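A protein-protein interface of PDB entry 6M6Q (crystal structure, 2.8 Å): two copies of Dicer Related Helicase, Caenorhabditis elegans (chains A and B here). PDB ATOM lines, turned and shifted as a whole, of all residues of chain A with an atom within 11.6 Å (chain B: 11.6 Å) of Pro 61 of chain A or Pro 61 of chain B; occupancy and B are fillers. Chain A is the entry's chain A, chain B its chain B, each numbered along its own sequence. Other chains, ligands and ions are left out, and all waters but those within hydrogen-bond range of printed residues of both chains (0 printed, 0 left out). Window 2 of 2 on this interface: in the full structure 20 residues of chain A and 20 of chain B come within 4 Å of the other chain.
Ser 57 of chain A touches Pro 60 of chain B, and with the chains exchanged Pro 60 of chain A touches Ser 57 of chain B.
Leu 58 of chain A touches Pro 60 of chain B, and with the chains exchanged Pro 60 of chain A touches Leu 58 of chain B.
Phe 59 of chain A touches Pro 60 of chain B, and with the chains exchanged Pro 60 of chain A touches Phe 59 of chain B.
Pro 61 of chain B touches its own counterpart, Pro 61 of chain A.
18 positions are printed for both chains.
Of the 7 pairs that touch across the chains among the printed residues, 7 have their exchanged pair printed and touching as well.
Among the printed residues, pairs that only touch across the chains: Ser 57 of chain A with Pro 60 of chain B (3.3 Å), Leu 58 of chain A with Pro 60 of chain B (3.3 Å), Phe 59 of chain A with Pro 60 of chain B (3.6 Å), Pro 60 of chain A with Ser 57 of chain B (3.4 Å), Pro 60 of chain A with Leu 58 of chain B (3.6 Å), Pro 60 of chain A with Phe 59 of chain B (3.6 Å) and Pro 61 of chain A with Pro 61 of chain B (3.9 Å).
Pro 61 of chain A touches just one residue of chain B: Pro 61.
Pro 61 of chain B touches just one residue of chain A: Pro 61 (3.9 Å).
No residue of chain A comes within 4 Å of Gly 62 of chain B.
Printed residues of chain A within 4 Å of Leu 58 of chain B: Pro 60.
Of the printed residues of chain B, Leu 58 of chain A touches Pro 60.
Of the printed residues of chain B, Ser 57 of chain A touches Pro 60.
Printed residues of chain A within 4 Å of Phe 59 of chain B: Pro 60.
Of the printed residues of chain B, Phe 59 of chain A touches Pro 60.
The nearest residue of chain A that does not touch Pro 61 of chain B is Phe 59 of chain A (4.7 Å).
Printed residues of chain B that touch a printed residue of chain A: Ser 57, Leu 58, Phe 59, Pro 60 and Pro 61.
Hydrophobic or aromatic side chains of chain B within 4 Å of the printed part of chain A: Pro 60 and Pro 61.
Of the 19 printed residues of chain A, 5 touch a printed residue of chain B.
Printed residues of chain A that touch a printed residue of chain B: Ser 57, Leu 58, Phe 59, Pro 60 and Pro 61.
Among the printed residues, 7 pairs touch across the chains.
Among the printed residues, no Asp or Glu carboxylate lies within 4 Å of a Lys or Arg side-chain nitrogen of the other chain.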
ATOM      1  N   ILE A  49      14.903 -20.525  24.783  1.00  0.00           N
ATOM      2  CA  ILE A  49      15.561 -21.450  23.812  1.00  0.00           C
ATOM      3  C   ILE A  49      16.974 -21.793  24.299  1.00  0.00           C
ATOM      4  O   ILE A  49      17.628 -22.617  23.642  1.00  0.00           O
ATOM      5  CB  ILE A  49      15.570 -20.822  22.395  1.00  0.00           C
ATOM      6  CG1 ILE A  49      16.392 -19.525  22.348  1.00  0.00           C
ATOM      7  CG2 ILE A  49      14.138 -20.611  21.897  1.00  0.00           C
ATOM      8  CD1 ILE A  49      16.400 -18.829  21.006  1.00  0.00           C
ATOM      9  N   LYS A  53      20.108 -19.935  20.917  1.00  0.00           N
ATOM     10  CA  LYS A  53      20.153 -18.509  20.483  1.00  0.00           C
ATOM     11  C   LYS A  53      21.562 -18.139  19.977  1.00  0.00           C
ATOM     12  O   LYS A  53      21.662 -17.211  19.163  1.00  0.00           O
ATOM     13  CB  LYS A  53      19.738 -17.588  21.635  1.00  0.00           C
ATOM     14  CG  LYS A  53      19.525 -16.137  21.237  1.00  0.00           C
ATOM     15  CD  LYS A  53      18.535 -15.396  22.111  1.00  0.00           C
ATOM     16  CE  LYS A  53      18.662 -13.891  21.998  1.00  0.00           C
ATOM     17  NZ  LYS A  53      18.587 -13.438  20.586  1.00  0.00           N
ATOM     18  N   PHE A  55      23.235 -19.468  17.858  1.00  0.00           N
ATOM     19  CA  PHE A  55      23.347 -19.921  16.439  1.00  0.00           C
ATOM     20  C   PHE A  55      22.421 -19.101  15.531  1.00  0.00           C
ATOM     21  O   PHE A  55      22.331 -19.416  14.319  1.00  0.00           O
ATOM     22  CB  PHE A  55      23.049 -21.414  16.336  1.00  0.00           C
ATOM     23  CG  PHE A  55      24.013 -22.290  17.085  1.00  0.00           C
ATOM     24  CD1 PHE A  55      23.757 -22.674  18.387  1.00  0.00           C
ATOM     25  CD2 PHE A  55      25.181 -22.725  16.489  1.00  0.00           C
ATOM     26  CE1 PHE A  55      24.635 -23.507  19.069  1.00  0.00           C
ATOM     27  CE2 PHE A  55      26.069 -23.540  17.174  1.00  0.00           C
ATOM     28  CZ  PHE A  55      25.788 -23.945  18.456  1.00  0.00           C
ATOM     29  N   GLU A  56      21.840 -18.031  16.076  1.00  0.00           N
ATOM     30  CA  GLU A  56      20.825 -17.157  15.420  1.00  0.00           C
ATOM     31  C   GLU A  56      21.318 -16.704  14.036  1.00  0.00           C
ATOM     32  O   GLU A  56      20.486 -16.643  13.090  1.00  0.00           O
ATOM     33  CB  GLU A  56      20.567 -15.939  16.316  1.00  0.00           C
ATOM     34  CG  GLU A  56      19.184 -15.337  16.183  1.00  0.00           C
ATOM     35  CD  GLU A  56      18.914 -14.218  17.178  1.00  0.00           C
ATOM     36  OE1 GLU A  56      19.891 -13.687  17.745  1.00  0.00           O
ATOM     37  OE2 GLU A  56      17.734 -13.884  17.388  1.00  0.00           O
ATOM     38  N   SER A  57      22.601 -16.341  13.934  1.00  0.00           N
ATOM     39  CA  SER A  57      23.192 -15.627  12.766  1.00  0.00           C
ATOM     40  C   SER A  57      23.265 -16.559  11.553  1.00  0.00           C
ATOM     41  O   SER A  57      23.376 -16.032  10.411  1.00  0.00           O
ATOM     42  CB  SER A  57      24.547 -15.070  13.101  1.00  0.00           C
ATOM     43  OG  SER A  57      25.471 -16.110  13.374  1.00  0.00           O
ATOM     44  N   LEU A  58      23.196 -17.879  11.787  1.00  0.00           N
ATOM     45  CA  LEU A  58      23.416 -18.929  10.759  1.00  0.00           C
ATOM     46  C   LEU A  58      22.102 -19.278  10.041  1.00  0.00           C
ATOM     47  O   LEU A  58      22.154 -20.073   9.080  1.00  0.00           O
ATOM     48  CB  LEU A  58      24.023 -20.143  11.447  1.00  0.00           C
ATOM     49  CG  LEU A  58      25.502 -19.984  11.797  1.00  0.00           C
ATOM     50  CD1 LEU A  58      25.770 -20.336  13.252  1.00  0.00           C
ATOM     51  CD2 LEU A  58      26.372 -20.827  10.877  1.00  0.00           C
ATOM     52  N   PHE A  59      20.987 -18.674  10.459  1.00  0.00           N
ATOM     53  CA  PHE A  59      19.660 -18.830   9.820  1.00  0.00           C
ATOM     54  C   PHE A  59      19.118 -17.466   9.457  1.00  0.00           C
ATOM     55  O   PHE A  59      19.604 -16.460   9.948  1.00  0.00           O
ATOM     56  CB  PHE A  59      18.684 -19.528  10.755  1.00  0.00           C
ATOM     57  CG  PHE A  59      19.186 -20.806  11.361  1.00  0.00           C
ATOM     58  CD1 PHE A  59      20.136 -20.790  12.367  1.00  0.00           C
ATOM     59  CD2 PHE A  59      18.682 -22.024  10.951  1.00  0.00           C
ATOM     60  CE1 PHE A  59      20.590 -21.971  12.931  1.00  0.00           C
ATOM     61  CE2 PHE A  59      19.113 -23.201  11.538  1.00  0.00           C
ATOM     62  CZ  PHE A  59      20.073 -23.176  12.518  1.00  0.00           C
ATOM     63  N   PRO A  60      18.047 -17.389   8.655  1.00  0.00           N
ATOM     64  CA  PRO A  60      17.408 -16.113   8.362  1.00  0.00           C
ATOM     65  C   PRO A  60      16.704 -15.601   9.612  1.00  0.00           C
ATOM     66  O   PRO A  60      16.279 -16.392  10.450  1.00  0.00           O
ATOM     67  CB  PRO A  60      16.413 -16.435   7.235  1.00  0.00           C
ATOM     68  CG  PRO A  60      16.789 -17.855   6.784  1.00  0.00           C
ATOM     69  CD  PRO A  60      17.381 -18.514   8.008  1.00  0.00           C
ATOM     70  N   PRO A  61      16.551 -14.273   9.765  1.00  0.00           N
ATOM     71  CA  PRO A  61      15.983 -13.694  10.987  1.00  0.00           C
ATOM     72  C   PRO A  61      14.659 -14.350  11.423  1.00  0.00           C
ATOM     73  O   PRO A  61      13.692 -14.332  10.662  1.00  0.00           O
ATOM     74  CB  PRO A  61      15.774 -12.213  10.614  1.00  0.00           C
ATOM     75  CG  PRO A  61      15.853 -12.187   9.091  1.00  0.00           C
ATOM     76  CD  PRO A  61      16.849 -13.264   8.746  1.00  0.00           C
ATOM     77  N   GLY A  62      14.639 -14.899  12.636  1.00  0.00           N
ATOM     78  CA  GLY A  62      13.451 -15.539  13.225  1.00  0.00           C
ATOM     79  C   GLY A  62      13.509 -17.044  13.097  1.00  0.00           C
ATOM     80  O   GLY A  62      13.048 -17.732  14.032  1.00  0.00           O
ATOM     81  N   LYS A  63      14.069 -17.545  11.990  1.00  0.00           N
ATOM     82  CA  LYS A  63      14.118 -18.992  11.656  1.00  0.00           C
ATOM     83  C   LYS A  63      14.640 -19.785  12.857  1.00  0.00           C
ATOM     84  O   LYS A  63      14.000 -20.789  13.224  1.00  0.00           O
ATOM     85  CB  LYS A  63      14.996 -19.232  10.429  1.00  0.00           C
ATOM     86  CG  LYS A  63      14.338 -18.876   9.107  1.00  0.00           C
ATOM     87  CD  LYS A  63      13.259 -19.865   8.713  1.00  0.00           C
ATOM     88  CE  LYS A  63      12.023 -19.205   8.137  1.00  0.00           C
ATOM     89  NZ  LYS A  63      10.783 -19.787   8.702  1.00  0.00           N
ATOM     90  N   LEU A  64      15.739 -19.348  13.462  1.00  0.00           N
ATOM     91  CA  LEU A  64      16.323 -20.058  14.621  1.00  0.00           C
ATOM     92  C   LEU A  64      15.255 -20.191  15.715  1.00  0.00           C
ATOM     93  O   LEU A  64      15.140 -21.284  16.276  1.00  0.00           O
ATOM     94  CB  LEU A  64      17.560 -19.323  15.136  1.00  0.00           C
ATOM     95  CG  LEU A  64      18.388 -20.111  16.156  1.00  0.00           C
ATOM     96  CD1 LEU A  64      17.697 -20.170  17.513  1.00  0.00           C
ATOM     97  CD2 LEU A  64      18.667 -21.518  15.660  1.00  0.00           C
ATOM     98  N   GLU A  65      14.496 -19.124  15.986  1.00  0.00           N
ATOM     99  CA  GLU A  65      13.434 -19.118  17.032  1.00  0.00           C
ATOM    100  C   GLU A  65      12.418 -20.233  16.732  1.00  0.00           C
ATOM    101  O   GLU A  65      12.111 -21.003  17.660  1.00  0.00           O
ATOM    102  CB  GLU A  65      12.761 -17.743  17.142  1.00  0.00           C
ATOM    103  CG  GLU A  65      11.733 -17.641  18.271  1.00  0.00           C
ATOM    104  CD  GLU A  65      12.285 -17.491  19.690  1.00  0.00           C
ATOM    105  OE1 GLU A  65      11.477 -17.506  20.635  1.00  0.00           O
ATOM    106  OE2 GLU A  65      13.517 -17.381  19.846  1.00  0.00           O
ATOM    107  N   GLU A  66      11.909 -20.304  15.497  1.00  0.00           N
ATOM    108  CA  GLU A  66      10.896 -21.317  15.075  1.00  0.00           C
ATOM    109  C   GLU A  66      11.468 -22.720  15.313  1.00  0.00           C
ATOM    110  O   GLU A  66      10.775 -23.548  15.921  1.00  0.00           O
ATOM    111  CB  GLU A  66      10.509 -21.155  13.597  1.00  0.00           C
ATOM    112  CG  GLU A  66       9.772 -19.859  13.264  1.00  0.00           C
ATOM    113  CD  GLU A  66       9.552 -19.648  11.768  1.00  0.00           C
ATOM    114  OE1 GLU A  66       9.637 -20.662  11.000  1.00  0.00           O
ATOM    115  OE2 GLU A  66       9.315 -18.477  11.356  1.00  0.00           O
ATOM    116  N   ILE A  67      12.671 -22.984  14.801  1.00  0.00           N
ATOM    117  CA  ILE A  67      13.293 -24.339  14.775  1.00  0.00           C
ATOM    118  C   ILE A  67      13.467 -24.826  16.214  1.00  0.00           C
ATOM    119  O   ILE A  67      12.929 -25.896  16.545  1.00  0.00           O
ATOM    120  CB  ILE A  67      14.619 -24.306  13.995  1.00  0.00           C
ATOM    121  CG1 ILE A  67      14.361 -24.181  12.491  1.00  0.00           C
ATOM    122  CG2 ILE A  67      15.480 -25.515  14.323  1.00  0.00           C
ATOM    123  CD1 ILE A  67      15.428 -23.442  11.740  1.00  0.00           C
ATOM    124  N   ALA A  68      14.132 -24.026  17.048  1.00  0.00           N
ATOM    125  CA  ALA A  68      14.338 -24.292  18.491  1.00  0.00           C
ATOM    126  C   ALA A  68      12.995 -24.645  19.135  1.00  0.00           C
ATOM    127  O   ALA A  68      12.920 -25.702  19.771  1.00  0.00           O
ATOM    128  CB  ALA A  68      14.983 -23.098  19.159  1.00  0.00           C
ATOM    129  N   THR A 126      22.557 -27.533   9.625  1.00  0.00           N
ATOM    130  CA  THR A 126      22.876 -26.117   9.295  1.00  0.00           C
ATOM    131  C   THR A 126      24.143 -25.690  10.045  1.00  0.00           C
ATOM    132  O   THR A 126      25.048 -25.092   9.392  1.00  0.00           O
ATOM    133  CB  THR A 126      21.701 -25.182   9.584  1.00  0.00           C
ATOM    134  OG1 THR A 126      20.585 -25.626   8.818  1.00  0.00           O
ATOM    135  CG2 THR A 126      21.990 -23.740   9.227  1.00  0.00           C
ATOM    136  N   ASP A 130      29.143 -26.024   8.718  1.00  0.00           N
ATOM    137  CA  ASP A 130      29.622 -24.639   8.437  1.00  0.00           C
ATOM    138  C   ASP A 130      30.696 -24.292   9.474  1.00  0.00           C
ATOM    139  O   ASP A 130      30.504 -24.659  10.671  1.00  0.00           O
ATOM    140  CB  ASP A 130      28.470 -23.637   8.517  1.00  0.00           C
ATOM    141  CG  ASP A 130      28.831 -22.191   8.196  1.00  0.00           C
ATOM    142  OD1 ASP A 130      29.122 -21.414   9.146  1.00  0.00           O
ATOM    143  OD2 ASP A 130      28.726 -21.822   7.023  1.00  0.00           O
ATOM    144  N   LYS A 132      31.851 -21.355  10.872  1.00  0.00           N
ATOM    145  CA  LYS A 132      31.397 -20.439  11.962  1.00  0.00           C
ATOM    146  C   LYS A 132      30.497 -21.231  12.932  1.00  0.00           C
ATOM    147  O   LYS A 132      30.733 -21.176  14.238  1.00  0.00           O
ATOM    148  CB  LYS A 132      30.698 -19.209  11.358  1.00  0.00           C
ATOM    149  CG  LYS A 132      31.614 -18.016  11.084  1.00  0.00           C
ATOM    150  CD  LYS A 132      31.056 -17.027  10.091  1.00  0.00           C
ATOM    151  CE  LYS A 132      32.126 -16.397   9.230  1.00  0.00           C
ATOM    152  NZ  LYS A 132      31.541 -15.744   8.039  1.00  0.00           N
ATOM    153  N   ILE B  49      22.643 -10.539  -9.866  1.00  0.00           N
ATOM    154  CA  ILE B  49      22.585 -11.979  -9.486  1.00  0.00           C
ATOM    155  C   ILE B  49      21.306 -12.592 -10.074  1.00  0.00           C
ATOM    156  O   ILE B  49      21.092 -13.791  -9.883  1.00  0.00           O
ATOM    157  CB  ILE B  49      22.705 -12.172  -7.955  1.00  0.00           C
ATOM    158  CG1 ILE B  49      21.568 -11.500  -7.185  1.00  0.00           C
ATOM    159  CG2 ILE B  49      24.073 -11.703  -7.461  1.00  0.00           C
ATOM    160  CD1 ILE B  49      21.442 -11.967  -5.747  1.00  0.00           C
ATOM    161  N   LYS B  53      18.169 -13.781  -6.591  1.00  0.00           N
ATOM    162  CA  LYS B  53      17.783 -12.780  -5.557  1.00  0.00           C
ATOM    163  C   LYS B  53      16.409 -13.135  -4.967  1.00  0.00           C
ATOM    164  O   LYS B  53      16.178 -12.794  -3.796  1.00  0.00           O
ATOM    165  CB  LYS B  53      17.784 -11.363  -6.128  1.00  0.00           C
ATOM    166  CG  LYS B  53      18.108 -10.279  -5.114  1.00  0.00           C
ATOM    167  CD  LYS B  53      17.837  -8.882  -5.608  1.00  0.00           C
ATOM    168  CE  LYS B  53      18.287  -7.824  -4.624  1.00  0.00           C
ATOM    169  NZ  LYS B  53      17.586  -7.956  -3.324  1.00  0.00           N
ATOM    170  N   PHE B  55      15.458 -15.685  -3.753  1.00  0.00           N
ATOM    171  CA  PHE B  55      15.655 -16.748  -2.725  1.00  0.00           C
ATOM    172  C   PHE B  55      16.364 -16.175  -1.486  1.00  0.00           C
ATOM    173  O   PHE B  55      16.687 -16.957  -0.565  1.00  0.00           O
ATOM    174  CB  PHE B  55      16.422 -17.931  -3.327  1.00  0.00           C
ATOM    175  CG  PHE B  55      15.746 -18.580  -4.511  1.00  0.00           C
ATOM    176  CD1 PHE B  55      15.998 -18.142  -5.800  1.00  0.00           C
ATOM    177  CD2 PHE B  55      14.855 -19.624  -4.336  1.00  0.00           C
ATOM    178  CE1 PHE B  55      15.359 -18.720  -6.885  1.00  0.00           C
ATOM    179  CE2 PHE B  55      14.222 -20.206  -5.423  1.00  0.00           C
ATOM    180  CZ  PHE B  55      14.471 -19.748  -6.693  1.00  0.00           C
ATOM    181  N   GLU B  56      16.544 -14.851  -1.431  1.00  0.00           N
ATOM    182  CA  GLU B  56      17.368 -14.182  -0.381  1.00  0.00           C
ATOM    183  C   GLU B  56      16.739 -14.384   1.016  1.00  0.00           C
ATOM    184  O   GLU B  56      17.512 -14.439   1.994  1.00  0.00           O
ATOM    185  CB  GLU B  56      17.615 -12.710  -0.727  1.00  0.00           C
ATOM    186  CG  GLU B  56      16.373 -11.840  -0.727  1.00  0.00           C
ATOM    187  CD  GLU B  56      16.588 -10.463  -1.348  1.00  0.00           C
ATOM    188  OE1 GLU B  56      15.581  -9.829  -1.760  1.00  0.00           O
ATOM    189  OE2 GLU B  56      17.768 -10.023  -1.435  1.00  0.00           O
ATOM    190  N   SER B  57      15.418 -14.575   1.101  1.00  0.00           N
ATOM    191  CA  SER B  57      14.658 -14.766   2.369  1.00  0.00           C
ATOM    192  C   SER B  57      15.027 -16.101   3.037  1.00  0.00           C
ATOM    193  O   SER B  57      14.774 -16.241   4.273  1.00  0.00           O
ATOM    194  CB  SER B  57      13.189 -14.686   2.123  1.00  0.00           C
ATOM    195  OG  SER B  57      12.860 -15.222   0.849  1.00  0.00           O
ATOM    196  N   LEU B  58      15.609 -17.037   2.271  1.00  0.00           N
ATOM    197  CA  LEU B  58      15.884 -18.433   2.711  1.00  0.00           C
ATOM    198  C   LEU B  58      17.314 -18.561   3.250  1.00  0.00           C
ATOM    199  O   LEU B  58      17.666 -19.660   3.706  1.00  0.00           O
ATOM    200  CB  LEU B  58      15.666 -19.383   1.535  1.00  0.00           C
ATOM    201  CG  LEU B  58      14.216 -19.562   1.099  1.00  0.00           C
ATOM    202  CD1 LEU B  58      14.156 -19.973  -0.353  1.00  0.00           C
ATOM    203  CD2 LEU B  58      13.497 -20.578   1.983  1.00  0.00           C
ATOM    204  N   PHE B  59      18.102 -17.491   3.234  1.00  0.00           N
ATOM    205  CA  PHE B  59      19.480 -17.494   3.787  1.00  0.00           C
ATOM    206  C   PHE B  59      19.635 -16.348   4.766  1.00  0.00           C
ATOM    207  O   PHE B  59      18.853 -15.410   4.743  1.00  0.00           O
ATOM    208  CB  PHE B  59      20.520 -17.375   2.680  1.00  0.00           C
ATOM    209  CG  PHE B  59      20.399 -18.393   1.578  1.00  0.00           C
ATOM    210  CD1 PHE B  59      19.577 -18.157   0.483  1.00  0.00           C
ATOM    211  CD2 PHE B  59      21.128 -19.574   1.616  1.00  0.00           C
ATOM    212  CE1 PHE B  59      19.498 -19.072  -0.556  1.00  0.00           C
ATOM    213  CE2 PHE B  59      21.032 -20.494   0.585  1.00  0.00           C
ATOM    214  CZ  PHE B  59      20.227 -20.235  -0.503  1.00  0.00           C
ATOM    215  N   PRO B  60      20.660 -16.385   5.640  1.00  0.00           N
ATOM    216  CA  PRO B  60      20.965 -15.263   6.516  1.00  0.00           C
ATOM    217  C   PRO B  60      21.368 -14.041   5.713  1.00  0.00           C
ATOM    218  O   PRO B  60      21.961 -14.177   4.653  1.00  0.00           O
ATOM    219  CB  PRO B  60      22.144 -15.762   7.360  1.00  0.00           C
ATOM    220  CG  PRO B  60      22.009 -17.263   7.303  1.00  0.00           C
ATOM    221  CD  PRO B  60      21.521 -17.536   5.899  1.00  0.00           C
ATOM    222  N   PRO B  61      21.064 -12.820   6.207  1.00  0.00           N
ATOM    223  CA  PRO B  61      21.298 -11.582   5.455  1.00  0.00           C
ATOM    224  C   PRO B  61      22.684 -11.497   4.792  1.00  0.00           C
ATOM    225  O   PRO B  61      23.691 -11.563   5.476  1.00  0.00           O
ATOM    226  CB  PRO B  61      21.141 -10.488   6.529  1.00  0.00           C
ATOM    227  CG  PRO B  61      21.199 -11.249   7.857  1.00  0.00           C
ATOM    228  CD  PRO B  61      20.535 -12.561   7.548  1.00  0.00           C
ATOM    229  N   GLY B  62      22.704 -11.382   3.470  1.00  0.00           N
ATOM    230  CA  GLY B  62      23.941 -11.237   2.689  1.00  0.00           C
ATOM    231  C   GLY B  62      24.528 -12.572   2.250  1.00  0.00           C
ATOM    232  O   GLY B  62      25.288 -12.560   1.298  1.00  0.00           O
ATOM    233  N   LYS B  63      24.192 -13.679   2.917  1.00  0.00           N
ATOM    234  CA  LYS B  63      24.707 -15.022   2.559  1.00  0.00           C
ATOM    235  C   LYS B  63      24.293 -15.386   1.121  1.00  0.00           C
ATOM    236  O   LYS B  63      25.095 -16.050   0.432  1.00  0.00           O
ATOM    237  CB  LYS B  63      24.234 -16.081   3.552  1.00  0.00           C
ATOM    238  CG  LYS B  63      24.771 -17.481   3.283  1.00  0.00           C
ATOM    239  CD  LYS B  63      25.465 -18.111   4.484  1.00  0.00           C
ATOM    240  CE  LYS B  63      26.472 -19.176   4.096  1.00  0.00           C
ATOM    241  NZ  LYS B  63      27.848 -18.625   3.974  1.00  0.00           N
ATOM    242  N   LEU B  64      23.090 -15.021   0.683  1.00  0.00           N
ATOM    243  CA  LEU B  64      22.619 -15.372  -0.681  1.00  0.00           C
ATOM    244  C   LEU B  64      23.603 -14.795  -1.695  1.00  0.00           C
ATOM    245  O   LEU B  64      24.186 -15.575  -2.447  1.00  0.00           O
ATOM    246  CB  LEU B  64      21.205 -14.839  -0.916  1.00  0.00           C
ATOM    247  CG  LEU B  64      20.511 -15.339  -2.190  1.00  0.00           C
ATOM    248  CD1 LEU B  64      20.754 -14.400  -3.371  1.00  0.00           C
ATOM    249  CD2 LEU B  64      20.955 -16.748  -2.549  1.00  0.00           C
ATOM    250  N   GLU B  65      23.827 -13.482  -1.636  1.00  0.00           N
ATOM    251  CA  GLU B  65      24.743 -12.717  -2.538  1.00  0.00           C
ATOM    252  C   GLU B  65      26.112 -13.417  -2.608  1.00  0.00           C
ATOM    253  O   GLU B  65      26.591 -13.625  -3.730  1.00  0.00           O
ATOM    254  CB  GLU B  65      24.887 -11.272  -2.044  1.00  0.00           C
ATOM    255  CG  GLU B  65      25.797 -10.399  -2.903  1.00  0.00           C
ATOM    256  CD  GLU B  65      25.102  -9.672  -4.032  1.00  0.00           C
ATOM    257  OE1 GLU B  65      25.636  -8.633  -4.480  1.00  0.00           O
ATOM    258  OE2 GLU B  65      24.038 -10.139  -4.465  1.00  0.00           O
ATOM    259  N   GLU B  66      26.680 -13.827  -1.462  1.00  0.00           N
ATOM    260  CA  GLU B  66      27.981 -14.559  -1.407  1.00  0.00           C
ATOM    261  C   GLU B  66      27.889 -15.815  -2.291  1.00  0.00           C
ATOM    262  O   GLU B  66      28.803 -16.035  -3.108  1.00  0.00           O
ATOM    263  CB  GLU B  66      28.364 -14.944   0.030  1.00  0.00           C
ATOM    264  CG  GLU B  66      28.971 -13.817   0.850  1.00  0.00           C
ATOM    265  CD  GLU B  66      29.265 -14.215   2.292  1.00  0.00           C
ATOM    266  OE1 GLU B  66      29.453 -13.304   3.152  1.00  0.00           O
ATOM    267  OE2 GLU B  66      29.295 -15.442   2.561  1.00  0.00           O
ATOM    268  N   ILE B  67      26.850 -16.626  -2.097  1.00  0.00           N
ATOM    269  CA  ILE B  67      26.687 -17.935  -2.783  1.00  0.00           C
ATOM    270  C   ILE B  67      26.595 -17.685  -4.288  1.00  0.00           C
ATOM    271  O   ILE B  67      27.417 -18.267  -5.036  1.00  0.00           O
ATOM    272  CB  ILE B  67      25.472 -18.684  -2.232  1.00  0.00           C
ATOM    273  CG1 ILE B  67      25.766 -19.256  -0.842  1.00  0.00           C
ATOM    274  CG2 ILE B  67      25.027 -19.759  -3.199  1.00  0.00           C
ATOM    275  CD1 ILE B  67      24.556 -19.375   0.045  1.00  0.00           C
ATOM    276  N   ALA B  68      25.666 -16.821  -4.710  1.00  0.00           N
ATOM    277  CA  ALA B  68      25.444 -16.466  -6.127  1.00  0.00           C
ATOM    278  C   ALA B  68      26.788 -16.111  -6.761  1.00  0.00           C
ATOM    279  O   ALA B  68      27.149 -16.751  -7.740  1.00  0.00           O
ATOM    280  CB  ALA B  68      24.447 -15.338  -6.260  1.00  0.00           C
ATOM    281  N   THR B 126      19.327 -25.820  -0.065  1.00  0.00           N
ATOM    282  CA  THR B 126      18.613 -24.871   0.819  1.00  0.00           C
ATOM    283  C   THR B 126      17.203 -24.600   0.260  1.00  0.00           C
ATOM    284  O   THR B 126      16.238 -24.698   1.042  1.00  0.00           O
ATOM    285  CB  THR B 126      19.416 -23.574   1.009  1.00  0.00           C
ATOM    286  OG1 THR B 126      20.702 -23.888   1.534  1.00  0.00           O
ATOM    287  CG2 THR B 126      18.751 -22.610   1.959  1.00  0.00           C
ATOM    288  N   LYS B 132       8.462 -23.237   0.878  1.00  0.00           N
ATOM    289  CA  LYS B 132       8.420 -21.816   0.433  1.00  0.00           C
ATOM    290  C   LYS B 132       9.359 -21.652  -0.758  1.00  0.00           C
ATOM    291  O   LYS B 132       9.001 -20.919  -1.695  1.00  0.00           O
ATOM    292  CB  LYS B 132       8.807 -20.870   1.580  1.00  0.00           C
ATOM    293  CG  LYS B 132       8.061 -21.093   2.899  1.00  0.00           C
ATOM    294  CD  LYS B 132       8.550 -20.233   4.065  1.00  0.00           C
ATOM    295  CE  LYS B 132       9.927 -20.622   4.584  1.00  0.00           C
ATOM    296  NZ  LYS B 132       9.897 -21.864   5.398  1.00  0.00           N
